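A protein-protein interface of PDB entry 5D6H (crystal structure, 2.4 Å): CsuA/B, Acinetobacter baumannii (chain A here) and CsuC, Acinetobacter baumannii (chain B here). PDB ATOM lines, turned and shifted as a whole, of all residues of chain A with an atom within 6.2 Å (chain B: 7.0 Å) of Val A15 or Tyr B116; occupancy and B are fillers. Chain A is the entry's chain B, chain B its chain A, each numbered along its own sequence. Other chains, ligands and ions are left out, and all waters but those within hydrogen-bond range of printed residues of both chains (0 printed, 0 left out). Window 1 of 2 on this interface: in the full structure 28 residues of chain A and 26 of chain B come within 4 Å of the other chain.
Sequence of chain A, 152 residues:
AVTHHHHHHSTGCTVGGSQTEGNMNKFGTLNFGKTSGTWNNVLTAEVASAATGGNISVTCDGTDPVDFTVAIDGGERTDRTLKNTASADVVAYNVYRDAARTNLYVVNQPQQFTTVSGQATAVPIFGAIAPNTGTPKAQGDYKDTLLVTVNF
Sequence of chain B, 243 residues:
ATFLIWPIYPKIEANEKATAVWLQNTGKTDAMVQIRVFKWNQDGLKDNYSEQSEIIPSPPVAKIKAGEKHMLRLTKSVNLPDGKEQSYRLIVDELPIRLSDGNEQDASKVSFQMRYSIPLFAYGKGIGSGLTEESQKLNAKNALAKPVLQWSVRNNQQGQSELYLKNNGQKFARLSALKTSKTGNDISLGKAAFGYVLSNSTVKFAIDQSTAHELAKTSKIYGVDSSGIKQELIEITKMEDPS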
ATOM      1  N   CYS A  13      -4.264  -8.850 -24.434  1.00  0.00           N
ATOM      2  CA  CYS A  13      -4.086 -10.206 -23.952  1.00  0.00           C
ATOM      3  C   CYS A  13      -3.851 -10.227 -22.463  1.00  0.00           C
ATOM      4  O   CYS A  13      -3.140  -9.377 -21.931  1.00  0.00           O
ATOM      5  CB  CYS A  13      -2.923 -10.903 -24.666  1.00  0.00           C
ATOM      6  SG  CYS A  13      -3.198 -11.157 -26.402  1.00  0.00           S
ATOM      7  N   THR A  14      -4.463 -11.198 -21.797  1.00  0.00           N
ATOM      8  CA  THR A  14      -4.180 -11.454 -20.394  1.00  0.00           C
ATOM      9  C   THR A  14      -3.214 -12.616 -20.298  1.00  0.00           C
ATOM     10  O   THR A  14      -3.470 -13.686 -20.844  1.00  0.00           O
ATOM     11  CB  THR A  14      -5.444 -11.796 -19.602  1.00  0.00           C
ATOM     12  OG1 THR A  14      -6.290 -10.646 -19.546  1.00  0.00           O
ATOM     13  CG2 THR A  14      -5.081 -12.211 -18.184  1.00  0.00           C
ATOM     14  N   VAL A  15      -2.097 -12.396 -19.620  1.00  0.00           N
ATOM     15  CA  VAL A  15      -1.055 -13.395 -19.541  1.00  0.00           C
ATOM     16  C   VAL A  15      -0.744 -13.675 -18.090  1.00  0.00           C
ATOM     17  O   VAL A  15      -0.086 -12.890 -17.416  1.00  0.00           O
ATOM     18  CB  VAL A  15       0.230 -12.952 -20.255  1.00  0.00           C
ATOM     19  CG1 VAL A  15       1.165 -14.123 -20.391  1.00  0.00           C
ATOM     20  CG2 VAL A  15      -0.089 -12.391 -21.632  1.00  0.00           C
ATOM     21  N   GLY A  16      -1.226 -14.801 -17.596  1.00  0.00           N
ATOM     22  CA  GLY A  16      -1.010 -15.110 -16.202  1.00  0.00           C
ATOM     23  C   GLY A  16      -0.301 -16.423 -16.016  1.00  0.00           C
ATOM     24  O   GLY A  16       0.930 -16.469 -15.952  1.00  0.00           O
ATOM     25  N   GLY A  17      -1.090 -17.488 -15.917  1.00  0.00           N
ATOM     26  CA  GLY A  17      -2.537 -17.362 -15.955  1.00  0.00           C
ATOM     27  C   GLY A  17      -3.128 -17.060 -14.591  1.00  0.00           C
ATOM     28  O   GLY A  17      -2.420 -16.626 -13.681  1.00  0.00           O
ATOM     29  N   ILE A  56      -0.241 -21.783 -16.444  1.00  0.00           N
ATOM     30  CA  ILE A  56      -0.049 -20.499 -17.115  1.00  0.00           C
ATOM     31  C   ILE A  56      -0.929 -20.382 -18.358  1.00  0.00           C
ATOM     32  O   ILE A  56      -0.928 -21.276 -19.209  1.00  0.00           O
ATOM     33  CB  ILE A  56       1.430 -20.264 -17.475  1.00  0.00           C
ATOM     34  CG1 ILE A  56       2.307 -20.419 -16.220  1.00  0.00           C
ATOM     35  CG2 ILE A  56       1.598 -18.900 -18.128  1.00  0.00           C
ATOM     36  CD1 ILE A  56       3.718 -19.813 -16.316  1.00  0.00           C
ATOM     37  N   SER A  57      -1.697 -19.299 -18.458  1.00  0.00           N
ATOM     38  CA  SER A  57      -2.590 -19.130 -19.597  1.00  0.00           C
ATOM     39  C   SER A  57      -2.367 -17.825 -20.356  1.00  0.00           C
ATOM     40  O   SER A  57      -1.776 -16.869 -19.842  1.00  0.00           O
ATOM     41  CB  SER A  57      -4.055 -19.233 -19.173  1.00  0.00           C
ATOM     42  OG  SER A  57      -4.461 -18.066 -18.487  1.00  0.00           O
ATOM     43  N   VAL A  58      -2.834 -17.811 -21.598  1.00  0.00           N
ATOM     44  CA  VAL A  58      -2.817 -16.626 -22.416  1.00  0.00           C
ATOM     45  C   VAL A  58      -4.194 -16.505 -23.011  1.00  0.00           C
ATOM     46  O   VAL A  58      -4.705 -17.454 -23.580  1.00  0.00           O
ATOM     47  CB  VAL A  58      -1.788 -16.727 -23.537  1.00  0.00           C
ATOM     48  CG1 VAL A  58      -1.853 -15.486 -24.428  1.00  0.00           C
ATOM     49  CG2 VAL A  58      -0.398 -16.924 -22.969  1.00  0.00           C
ATOM     50  N   THR A  59      -4.803 -15.339 -22.877  1.00  0.00           N
ATOM     51  CA  THR A  59      -6.146 -15.130 -23.386  1.00  0.00           C
ATOM     52  C   THR A  59      -6.257 -13.773 -24.056  1.00  0.00           C
ATOM     53  O   THR A  59      -6.201 -12.729 -23.400  1.00  0.00           O
ATOM     54  CB  THR A  59      -7.186 -15.200 -22.268  1.00  0.00           C
ATOM     55  OG1 THR A  59      -6.874 -16.291 -21.395  1.00  0.00           O
ATOM     56  CG2 THR A  59      -8.581 -15.381 -22.854  1.00  0.00           C
ATOM     57  N   VAL A 148      10.545 -17.508 -18.111  1.00  0.00           N
ATOM     58  CA  VAL A 148       9.607 -17.790 -19.200  1.00  0.00           C
ATOM     59  C   VAL A 148       9.278 -16.515 -19.975  1.00  0.00           C
ATOM     60  O   VAL A 148       8.751 -15.544 -19.419  1.00  0.00           O
ATOM     61  CB  VAL A 148       8.311 -18.443 -18.688  1.00  0.00           C
ATOM     62  CG1 VAL A 148       7.427 -18.871 -19.828  1.00  0.00           C
ATOM     63  CG2 VAL A 148       8.641 -19.624 -17.783  1.00  0.00           C
ATOM     64  N   THR A 149       9.616 -16.530 -21.260  1.00  0.00           N
ATOM     65  CA  THR A 149       9.393 -15.405 -22.161  1.00  0.00           C
ATOM     66  C   THR A 149       8.218 -15.684 -23.069  1.00  0.00           C
ATOM     67  O   THR A 149       8.229 -16.648 -23.812  1.00  0.00           O
ATOM     68  CB  THR A 149      10.597 -15.193 -23.080  1.00  0.00           C
ATOM     69  OG1 THR A 149      11.752 -14.890 -22.288  1.00  0.00           O
ATOM     70  CG2 THR A 149      10.328 -14.048 -24.047  1.00  0.00           C
ATOM     71  N   VAL A 150       7.207 -14.843 -22.998  1.00  0.00           N
ATOM     72  CA  VAL A 150       6.056 -14.943 -23.857  1.00  0.00           C
ATOM     73  C   VAL A 150       6.233 -13.857 -24.887  1.00  0.00           C
ATOM     74  O   VAL A 150       6.312 -12.675 -24.536  1.00  0.00           O
ATOM     75  CB  VAL A 150       4.767 -14.715 -23.071  1.00  0.00           C
ATOM     76  CG1 VAL A 150       3.564 -14.921 -23.940  1.00  0.00           C
ATOM     77  CG2 VAL A 150       4.720 -15.647 -21.877  1.00  0.00           C
ATOM     78  N   ASN A 151       6.331 -14.259 -26.156  1.00  0.00           N
ATOM     79  CA  ASN A 151       6.533 -13.318 -27.250  1.00  0.00           C
ATOM     80  C   ASN A 151       5.320 -13.170 -28.139  1.00  0.00           C
ATOM     81  O   ASN A 151       4.812 -14.159 -28.682  1.00  0.00           O
ATOM     82  CB  ASN A 151       7.751 -13.695 -28.098  1.00  0.00           C
ATOM     83  CG  ASN A 151       9.051 -13.537 -27.349  1.00  0.00           C
ATOM     84  OD1 ASN A 151       9.237 -12.578 -26.629  1.00  0.00           O
ATOM     85  ND2 ASN A 151       9.949 -14.489 -27.502  1.00  0.00           N
ATOM     86  N   PHE A 152       4.857 -11.935 -28.288  1.00  0.00           N
ATOM     87  CA  PHE A 152       3.849 -11.644 -29.284  1.00  0.00           C
ATOM     88  C   PHE A 152       4.475 -11.117 -30.584  1.00  0.00           C
ATOM     89  O   PHE A 152       3.790 -10.720 -31.539  1.00  0.00           O
ATOM     90  CB  PHE A 152       2.808 -10.694 -28.727  1.00  0.00           C
ATOM     91  CG  PHE A 152       2.051 -11.263 -27.572  1.00  0.00           C
ATOM     92  CD1 PHE A 152       0.956 -12.083 -27.791  1.00  0.00           C
ATOM     93  CD2 PHE A 152       2.440 -10.994 -26.262  1.00  0.00           C
ATOM     94  CE1 PHE A 152       0.256 -12.617 -26.729  1.00  0.00           C
ATOM     95  CE2 PHE A 152       1.750 -11.520 -25.198  1.00  0.00           C
ATOM     96  CZ  PHE A 152       0.655 -12.340 -25.424  1.00  0.00           C
ATOM     97  OXT PHE A 152       5.704 -11.106 -30.722  1.00  0.00           O
ATOM     98  N   ALA B   1       2.992 -13.515 -11.377  1.00  0.00           N
ATOM     99  CA  ALA B   1       2.359 -12.262 -11.791  1.00  0.00           C
ATOM    100  C   ALA B   1       1.421 -12.510 -12.965  1.00  0.00           C
ATOM    101  O   ALA B   1       1.748 -13.273 -13.871  1.00  0.00           O
ATOM    102  CB  ALA B   1       3.415 -11.210 -12.170  1.00  0.00           C
ATOM    103  N   THR B   2       0.256 -11.868 -12.934  1.00  0.00           N
ATOM    104  CA  THR B   2      -0.709 -11.939 -14.022  1.00  0.00           C
ATOM    105  C   THR B   2      -1.007 -10.550 -14.606  1.00  0.00           C
ATOM    106  O   THR B   2      -1.588  -9.694 -13.934  1.00  0.00           O
ATOM    107  CB  THR B   2      -2.033 -12.539 -13.557  1.00  0.00           C
ATOM    108  OG1 THR B   2      -1.812 -13.844 -13.022  1.00  0.00           O
ATOM    109  CG2 THR B   2      -2.989 -12.638 -14.723  1.00  0.00           C
ATOM    110  N   PHE B   3      -0.637 -10.347 -15.866  1.00  0.00           N
ATOM    111  CA  PHE B   3      -0.833  -9.060 -16.515  1.00  0.00           C
ATOM    112  C   PHE B   3      -1.795  -9.073 -17.710  1.00  0.00           C
ATOM    113  O   PHE B   3      -1.676  -9.904 -18.622  1.00  0.00           O
ATOM    114  CB  PHE B   3       0.522  -8.490 -16.943  1.00  0.00           C
ATOM    115  CG  PHE B   3       1.389  -8.056 -15.791  1.00  0.00           C
ATOM    116  CD1 PHE B   3       1.157  -6.850 -15.144  1.00  0.00           C
ATOM    117  CD2 PHE B   3       2.440  -8.843 -15.359  1.00  0.00           C
ATOM    118  CE1 PHE B   3       1.954  -6.450 -14.078  1.00  0.00           C
ATOM    119  CE2 PHE B   3       3.246  -8.443 -14.291  1.00  0.00           C
ATOM    120  CZ  PHE B   3       2.994  -7.249 -13.655  1.00  0.00           C
ATOM    121  N   LEU B   4      -2.751  -8.148 -17.702  1.00  0.00           N
ATOM    122  CA  LEU B   4      -3.441  -7.790 -18.935  1.00  0.00           C
ATOM    123  C   LEU B   4      -2.627  -6.670 -19.591  1.00  0.00           C
ATOM    124  O   LEU B   4      -2.228  -5.708 -18.919  1.00  0.00           O
ATOM    125  CB  LEU B   4      -4.869  -7.325 -18.667  1.00  0.00           C
ATOM    126  CG  LEU B   4      -5.580  -6.611 -19.823  1.00  0.00           C
ATOM    127  CD1 LEU B   4      -5.732  -7.522 -21.060  1.00  0.00           C
ATOM    128  CD2 LEU B   4      -6.923  -6.108 -19.351  1.00  0.00           C
ATOM    129  N   ILE B   5      -2.390  -6.817 -20.892  1.00  0.00           N
ATOM    130  CA  ILE B   5      -1.563  -5.927 -21.689  1.00  0.00           C
ATOM    131  C   ILE B   5      -2.349  -5.451 -22.896  1.00  0.00           C
ATOM    132  O   ILE B   5      -2.774  -6.258 -23.731  1.00  0.00           O
ATOM    133  CB  ILE B   5      -0.336  -6.655 -22.275  1.00  0.00           C
ATOM    134  CG1 ILE B   5       0.450  -7.365 -21.189  1.00  0.00           C
ATOM    135  CG2 ILE B   5       0.568  -5.664 -23.010  1.00  0.00           C
ATOM    136  CD1 ILE B   5       1.647  -8.099 -21.735  1.00  0.00           C
ATOM    137  N   ILE B   8      -1.566  -5.124 -27.557  1.00  0.00           N
ATOM    138  CA  ILE B   8      -0.498  -6.075 -27.765  1.00  0.00           C
ATOM    139  C   ILE B   8       0.282  -5.738 -29.036  1.00  0.00           C
ATOM    140  O   ILE B   8       1.358  -6.267 -29.264  1.00  0.00           O
ATOM    141  CB  ILE B   8      -1.085  -7.500 -27.845  1.00  0.00           C
ATOM    142  CG1 ILE B   8      -0.121  -8.509 -27.239  1.00  0.00           C
ATOM    143  CG2 ILE B   8      -1.592  -7.847 -29.286  1.00  0.00           C
ATOM    144  CD1 ILE B   8      -0.224  -8.539 -25.739  1.00  0.00           C
ATOM    145  N   LEU B  23      -0.813  -1.739 -18.712  1.00  0.00           N
ATOM    146  CA  LEU B  23      -0.466  -2.962 -18.015  1.00  0.00           C
ATOM    147  C   LEU B  23      -1.276  -3.001 -16.761  1.00  0.00           C
ATOM    148  O   LEU B  23      -1.089  -2.167 -15.886  1.00  0.00           O
ATOM    149  CB  LEU B  23       0.998  -2.953 -17.601  1.00  0.00           C
ATOM    150  CG  LEU B  23       2.125  -3.004 -18.620  1.00  0.00           C
ATOM    151  CD1 LEU B  23       3.407  -3.298 -17.852  1.00  0.00           C
ATOM    152  CD2 LEU B  23       1.868  -4.064 -19.688  1.00  0.00           C
ATOM    153  N   THR B  26      -3.681  -8.094 -12.931  1.00  0.00           N
ATOM    154  CA  THR B  26      -4.957  -8.712 -12.566  1.00  0.00           C
ATOM    155  C   THR B  26      -4.773  -9.905 -11.618  1.00  0.00           C
ATOM    156  O   THR B  26      -5.578 -10.826 -11.626  1.00  0.00           O
ATOM    157  CB  THR B  26      -5.735  -9.196 -13.807  1.00  0.00           C
ATOM    158  OG1 THR B  26      -4.932 -10.140 -14.529  1.00  0.00           O
ATOM    159  CG2 THR B  26      -6.123  -8.009 -14.736  1.00  0.00           C
ATOM    160  N   VAL B  33       7.892  -4.357 -12.066  1.00  0.00           N
ATOM    161  CA  VAL B  33       8.350  -4.593 -13.419  1.00  0.00           C
ATOM    162  C   VAL B  33       9.427  -3.624 -13.897  1.00  0.00           C
ATOM    163  O   VAL B  33       9.451  -2.457 -13.513  1.00  0.00           O
ATOM    164  CB  VAL B  33       7.162  -4.592 -14.415  1.00  0.00           C
ATOM    165  CG1 VAL B  33       6.203  -5.723 -14.085  1.00  0.00           C
ATOM    166  CG2 VAL B  33       6.439  -3.276 -14.366  1.00  0.00           C
ATOM    167  N   GLN B  34      10.332  -4.135 -14.722  1.00  0.00           N
ATOM    168  CA  GLN B  34      11.262  -3.288 -15.429  1.00  0.00           C
ATOM    169  C   GLN B  34      10.775  -3.212 -16.863  1.00  0.00           C
ATOM    170  O   GLN B  34      10.377  -4.231 -17.460  1.00  0.00           O
ATOM    171  CB  GLN B  34      12.691  -3.847 -15.394  1.00  0.00           C
ATOM    172  CG  GLN B  34      13.666  -2.928 -16.122  1.00  0.00           C
ATOM    173  CD  GLN B  34      15.116  -3.365 -16.020  1.00  0.00           C
ATOM    174  OE1 GLN B  34      15.410  -4.506 -15.666  1.00  0.00           O
ATOM    175  NE2 GLN B  34      16.034  -2.451 -16.343  1.00  0.00           N
ATOM    176  N   ARG B  89      11.257  -3.990 -29.908  1.00  0.00           N
ATOM    177  CA  ARG B  89      10.539  -4.778 -28.912  1.00  0.00           C
ATOM    178  C   ARG B  89      10.389  -4.026 -27.596  1.00  0.00           C
ATOM    179  O   ARG B  89      11.358  -3.477 -27.048  1.00  0.00           O
ATOM    180  CB  ARG B  89      11.258  -6.098 -28.609  1.00  0.00           C
ATOM    181  CG  ARG B  89      11.684  -6.870 -29.824  1.00  0.00           C
ATOM    182  CD  ARG B  89      10.502  -7.467 -30.545  1.00  0.00           C
ATOM    183  NE  ARG B  89       9.702  -8.339 -29.695  1.00  0.00           N
ATOM    184  CZ  ARG B  89       8.784  -9.175 -30.168  1.00  0.00           C
ATOM    185  NH1 ARG B  89       8.576  -9.249 -31.468  1.00  0.00           N
ATOM    186  NH2 ARG B  89       8.070  -9.926 -29.351  1.00  0.00           N
ATOM    187  N   LEU B  90       9.169  -4.029 -27.077  1.00  0.00           N
ATOM    188  CA  LEU B  90       8.923  -3.546 -25.733  1.00  0.00           C
ATOM    189  C   LEU B  90       8.978  -4.751 -24.792  1.00  0.00           C
ATOM    190  O   LEU B  90       8.253  -5.722 -24.990  1.00  0.00           O
ATOM    191  CB  LEU B  90       7.576  -2.823 -25.651  1.00  0.00           C
ATOM    192  CG  LEU B  90       6.988  -2.630 -24.261  1.00  0.00           C
ATOM    193  CD1 LEU B  90       7.776  -1.578 -23.442  1.00  0.00           C
ATOM    194  CD2 LEU B  90       5.523  -2.247 -24.340  1.00  0.00           C
ATOM    195  N   ILE B  91       9.849  -4.667 -23.783  1.00  0.00           N
ATOM    196  CA  ILE B  91      10.118  -5.742 -22.845  1.00  0.00           C
ATOM    197  C   ILE B  91       9.720  -5.371 -21.411  1.00  0.00           C
ATOM    198  O   ILE B  91      10.218  -4.403 -20.844  1.00  0.00           O
ATOM    199  CB  ILE B  91      11.625  -6.117 -22.834  1.00  0.00           C
ATOM    200  CG1 ILE B  91      12.175  -6.314 -24.262  1.00  0.00           C
ATOM    201  CG2 ILE B  91      11.860  -7.318 -21.962  1.00  0.00           C
ATOM    202  CD1 ILE B  91      11.709  -7.593 -24.970  1.00  0.00           C
ATOM    203  N   VAL B  92       8.822  -6.169 -20.853  1.00  0.00           N
ATOM    204  CA  VAL B  92       8.382  -6.104 -19.486  1.00  0.00           C
ATOM    205  C   VAL B  92       8.946  -7.302 -18.715  1.00  0.00           C
ATOM    206  O   VAL B  92       8.666  -8.467 -19.051  1.00  0.00           O
ATOM    207  CB  VAL B  92       6.856  -6.149 -19.404  1.00  0.00           C
ATOM    208  CG1 VAL B  92       6.409  -6.062 -17.959  1.00  0.00           C
ATOM    209  CG2 VAL B  92       6.242  -5.047 -20.259  1.00  0.00           C
ATOM    210  N   ASP B  93       9.739  -7.006 -17.683  1.00  0.00           N
ATOM    211  CA  ASP B  93      10.365  -8.024 -16.844  1.00  0.00           C
ATOM    212  C   ASP B  93       9.751  -8.016 -15.456  1.00  0.00           C
ATOM    213  O   ASP B  93       9.667  -6.978 -14.825  1.00  0.00           O
ATOM    214  CB  ASP B  93      11.870  -7.791 -16.735  1.00  0.00           C
ATOM    215  CG  ASP B  93      12.630  -8.294 -17.951  1.00  0.00           C
ATOM    216  OD1 ASP B  93      12.300  -9.403 -18.430  1.00  0.00           O
ATOM    217  OD2 ASP B  93      13.560  -7.598 -18.432  1.00  0.00           O
ATOM    218  N   GLU B  94       9.302  -9.170 -14.988  1.00  0.00           N
ATOM    219  CA  GLU B  94       8.828  -9.289 -13.628  1.00  0.00           C
ATOM    220  C   GLU B  94      10.073  -9.377 -12.746  1.00  0.00           C
ATOM    221  O   GLU B  94      10.928 -10.228 -12.990  1.00  0.00           O
ATOM    222  CB  GLU B  94       7.979 -10.540 -13.483  1.00  0.00           C
ATOM    223  CG  GLU B  94       7.274 -10.683 -12.158  1.00  0.00           C
ATOM    224  CD  GLU B  94       6.794 -12.113 -11.906  1.00  0.00           C
ATOM    225  OE1 GLU B  94       7.075 -13.017 -12.735  1.00  0.00           O
ATOM    226  OE2 GLU B  94       6.144 -12.337 -10.861  1.00  0.00           O
ATOM    227  N   GLN B 113       9.418 -16.943 -13.379  1.00  0.00           N
ATOM    228  CA  GLN B 113       9.665 -15.501 -13.529  1.00  0.00           C
ATOM    229  C   GLN B 113       9.436 -14.998 -14.970  1.00  0.00           C
ATOM    230  O   GLN B 113      10.280 -15.201 -15.856  1.00  0.00           O
ATOM    231  CB  GLN B 113      11.084 -15.141 -13.078  1.00  0.00           C
ATOM    232  CG  GLN B 113      11.516 -13.730 -13.475  1.00  0.00           C
ATOM    233  CD  GLN B 113      12.878 -13.348 -12.920  1.00  0.00           C
ATOM    234  OE1 GLN B 113      13.293 -13.840 -11.867  1.00  0.00           O
ATOM    235  NE2 GLN B 113      13.577 -12.460 -13.623  1.00  0.00           N
ATOM    236  N   MET B 114       8.307 -14.320 -15.178  1.00  0.00           N
ATOM    237  CA  MET B 114       7.859 -13.921 -16.505  1.00  0.00           C
ATOM    238  C   MET B 114       8.608 -12.761 -17.145  1.00  0.00           C
ATOM    239  O   MET B 114       8.891 -11.750 -16.505  1.00  0.00           O
ATOM    240  CB  MET B 114       6.366 -13.574 -16.482  1.00  0.00           C
ATOM    241  CG  MET B 114       5.458 -14.578 -15.807  1.00  0.00           C
ATOM    242  SD  MET B 114       5.391 -16.306 -16.744  1.00  0.00           S
ATOM    243  CE  MET B 114       6.942 -17.124 -15.899  1.00  0.00           C
ATOM    244  N   ARG B 115       8.899 -12.922 -18.430  1.00  0.00           N
ATOM    245  CA  ARG B 115       9.216 -11.804 -19.306  1.00  0.00           C
ATOM    246  C   ARG B 115       8.219 -11.791 -20.462  1.00  0.00           C
ATOM    247  O   ARG B 115       7.963 -12.824 -21.099  1.00  0.00           O
ATOM    248  CB  ARG B 115      10.636 -11.899 -19.846  1.00  0.00           C
ATOM    249  CG  ARG B 115      10.822 -11.120 -21.136  1.00  0.00           C
ATOM    250  CD  ARG B 115      12.237 -11.241 -21.657  1.00  0.00           C
ATOM    251  NE  ARG B 115      13.201 -10.597 -20.779  1.00  0.00           N
ATOM    252  CZ  ARG B 115      14.421 -10.246 -21.171  1.00  0.00           C
ATOM    253  NH1 ARG B 115      14.806 -10.503 -22.416  1.00  0.00           N
ATOM    254  NH2 ARG B 115      15.248  -9.633 -20.332  1.00  0.00           N
ATOM    255  N   TYR B 116       7.624 -10.627 -20.692  1.00  0.00           N
ATOM    256  CA  TYR B 116       6.685 -10.427 -21.759  1.00  0.00           C
ATOM    257  C   TYR B 116       7.323  -9.479 -22.743  1.00  0.00           C
ATOM    258  O   TYR B 116       7.955  -8.481 -22.374  1.00  0.00           O
ATOM    259  CB  TYR B 116       5.383  -9.822 -21.244  1.00  0.00           C
ATOM    260  CG  TYR B 116       4.826 -10.489 -20.016  1.00  0.00           C
ATOM    261  CD1 TYR B 116       3.793 -11.403 -20.109  1.00  0.00           C
ATOM    262  CD2 TYR B 116       5.333 -10.202 -18.759  1.00  0.00           C
ATOM    263  CE1 TYR B 116       3.282 -12.015 -18.984  1.00  0.00           C
ATOM    264  CE2 TYR B 116       4.825 -10.807 -17.626  1.00  0.00           C
ATOM    265  CZ  TYR B 116       3.797 -11.716 -17.746  1.00  0.00           C
ATOM    266  OH  TYR B 116       3.285 -12.329 -16.625  1.00  0.00           O
ATOM    267  N   SER B 117       7.142  -9.782 -24.010  1.00  0.00           N
ATOM    268  CA  SER B 117       7.808  -9.061 -25.054  1.00  0.00           C
ATOM    269  C   SER B 117       6.786  -8.833 -26.169  1.00  0.00           C
ATOM    270  O   SER B 117       6.185  -9.783 -26.689  1.00  0.00           O
ATOM    271  CB  SER B 117       9.039  -9.867 -25.496  1.00  0.00           C
ATOM    272  OG  SER B 117       9.282  -9.759 -26.887  1.00  0.00           O
ATOM    273  N   ILE B 118       6.537  -7.571 -26.496  1.00  0.00           N
ATOM    274  CA  ILE B 118       5.554  -7.259 -27.528  1.00  0.00           C
ATOM    275  C   ILE B 118       6.179  -6.398 -28.618  1.00  0.00           C
ATOM    276  O   ILE B 118       7.144  -5.713 -28.364  1.00  0.00           O
ATOM    277  CB  ILE B 118       4.303  -6.590 -26.958  1.00  0.00           C
ATOM    278  CG1 ILE B 118       4.529  -5.106 -26.728  1.00  0.00           C
ATOM    279  CG2 ILE B 118       3.834  -7.289 -25.684  1.00  0.00           C
ATOM    280  CD1 ILE B 118       3.318  -4.453 -26.135  1.00  0.00           C
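Hydrophobic or aromatic side chains of chain A that line the printed part of chain B: Val A15, Ile A56, Val A148 and Phe A152.
Of the 22 printed residues of chain B, 12 touch a printed residue of chain A.
Hydrophobic or aromatic side chains of chain B within 4 Å of the printed part of chain A: Leu B4, Ile B5, Ile B8, Met B114 and Tyr B116.
Along chain B the printed residues that touch a printed residue of chain A span positions 1 to 117.
Among the printed residues, 25 pairs touch across the chains.
Among the printed residues, no Asp or Glu carboxylate lies within 4 Å of a Lys or Arg side-chain nitrogen of the other chain.
O of Ser A57 sits at hydrogen-bond distance from N of Gly A16.
NH2 of Arg B89 sits at hydrogen-bond distance from OG of Ser B117 (2.8 Å).
N of Glu B94 sits at hydrogen-bond distance from O of Met B114 (3.0 Å).
The backbone NH of Thr B26 is in hydrogen-bond range of the backbone carbonyl oxygen of Thr B2 (2.8 Å).
O of Ala B1 lies within hydrogen-bond range of OH of Tyr B116, at 3.3 Å.
The backbone NH (N) of Ala B1 sits close to the side-chain carboxylate (OE2) of Glu B94 (3.4 Å).
Among the printed residues, merely in contact across the chains: Thr A149 with Arg B115 (3.1 Å), Val A15 with Tyr B116 (3.3 Å), Cys A13 with Leu B4 (3.3 Å), Val A148 with Met B114 (3.4 Å), Thr A14 with Phe B3 (3.4 Å), Gly A16 with Thr B2 (3.5 Å), Thr A14 with Leu B4 (3.5 Å), Phe A152 with Ile B8 (3.5 Å), Val A15 with Thr B2 (3.6 Å), Val A150 with Tyr B116 (3.6 Å), Cys A13 with Phe B3 (3.7 Å), Cys A13 with Ile B8 (3.7 Å), Gly A16 with Ala B1 (3.9 Å), Ile A56 with Met B114 (3.9 Å) and Asn A151 with Arg B89 (3.98 Å).
Printed residues of chain B within 4 Å of Val A15: Thr B2 (3.6 Å), Phe B3 (2.7 Å) and Tyr B116 (3.3 Å).
Of the printed residues of chain A, Leu B4 touches Cys A13 (3.3 Å) and Thr A14 (3.5 Å).
Of the printed residues of chain B, Phe A152 touches Ile B8, Arg B89 and Ser B117.
Of the printed residues of chain B, Val A150 touches Arg B115, Tyr B116 and Ser B117.
Of the printed residues of chain A, Ile B8 touches Cys A13 and Phe A152.
Of the printed residues of chain A, Arg B115 touches Val A148, Thr A149 and Val A150.
Leu B23 touches none of the printed residues of chain A.
The nearest printed residue of chain A that does not touch Ala B1 is Val A15 (4.01 Å).
The backbone carbonyl oxygen (O) of Cys A13 sits at hydrogen-bond distance from the backbone NH (N) of Ile B5.
The side-chain hydroxyl of Thr B2 sits at hydrogen-bond distance from the backbone carbonyl oxygen of Gly A17 (2.9 Å).
The backbone NH (N) of Ser B117 lies within hydrogen-bond range of the backbone carbonyl oxygen (O) of Val A150.
O of Ser B117 lies within hydrogen-bond range of N of Phe A152, 3.0 Å away.
O of Gln B113 sits at hydrogen-bond distance from N of Val A148, 3.2 Å away.
O of Arg B115 lies within hydrogen-bond range of N of Val A150 (2.9 Å).
The chain-end carboxylate (OXT) of Phe A152 lies within salt-bridge range of the guanidinium group (NH2) of Arg B89, at 3.0 Å.
The backbone carbonyl oxygen of Phe B3 sits at hydrogen-bond distance from the backbone NH of Val A15, 2.7 Å away.
The side-chain hydroxyl (OG) of Ser B117 sits at hydrogen-bond distance from the side-chain amide oxygen (OD1) of Asn A151, 2.8 Å away.
N of Arg B115 is in hydrogen-bond range of O of Val A148 (2.8 Å).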
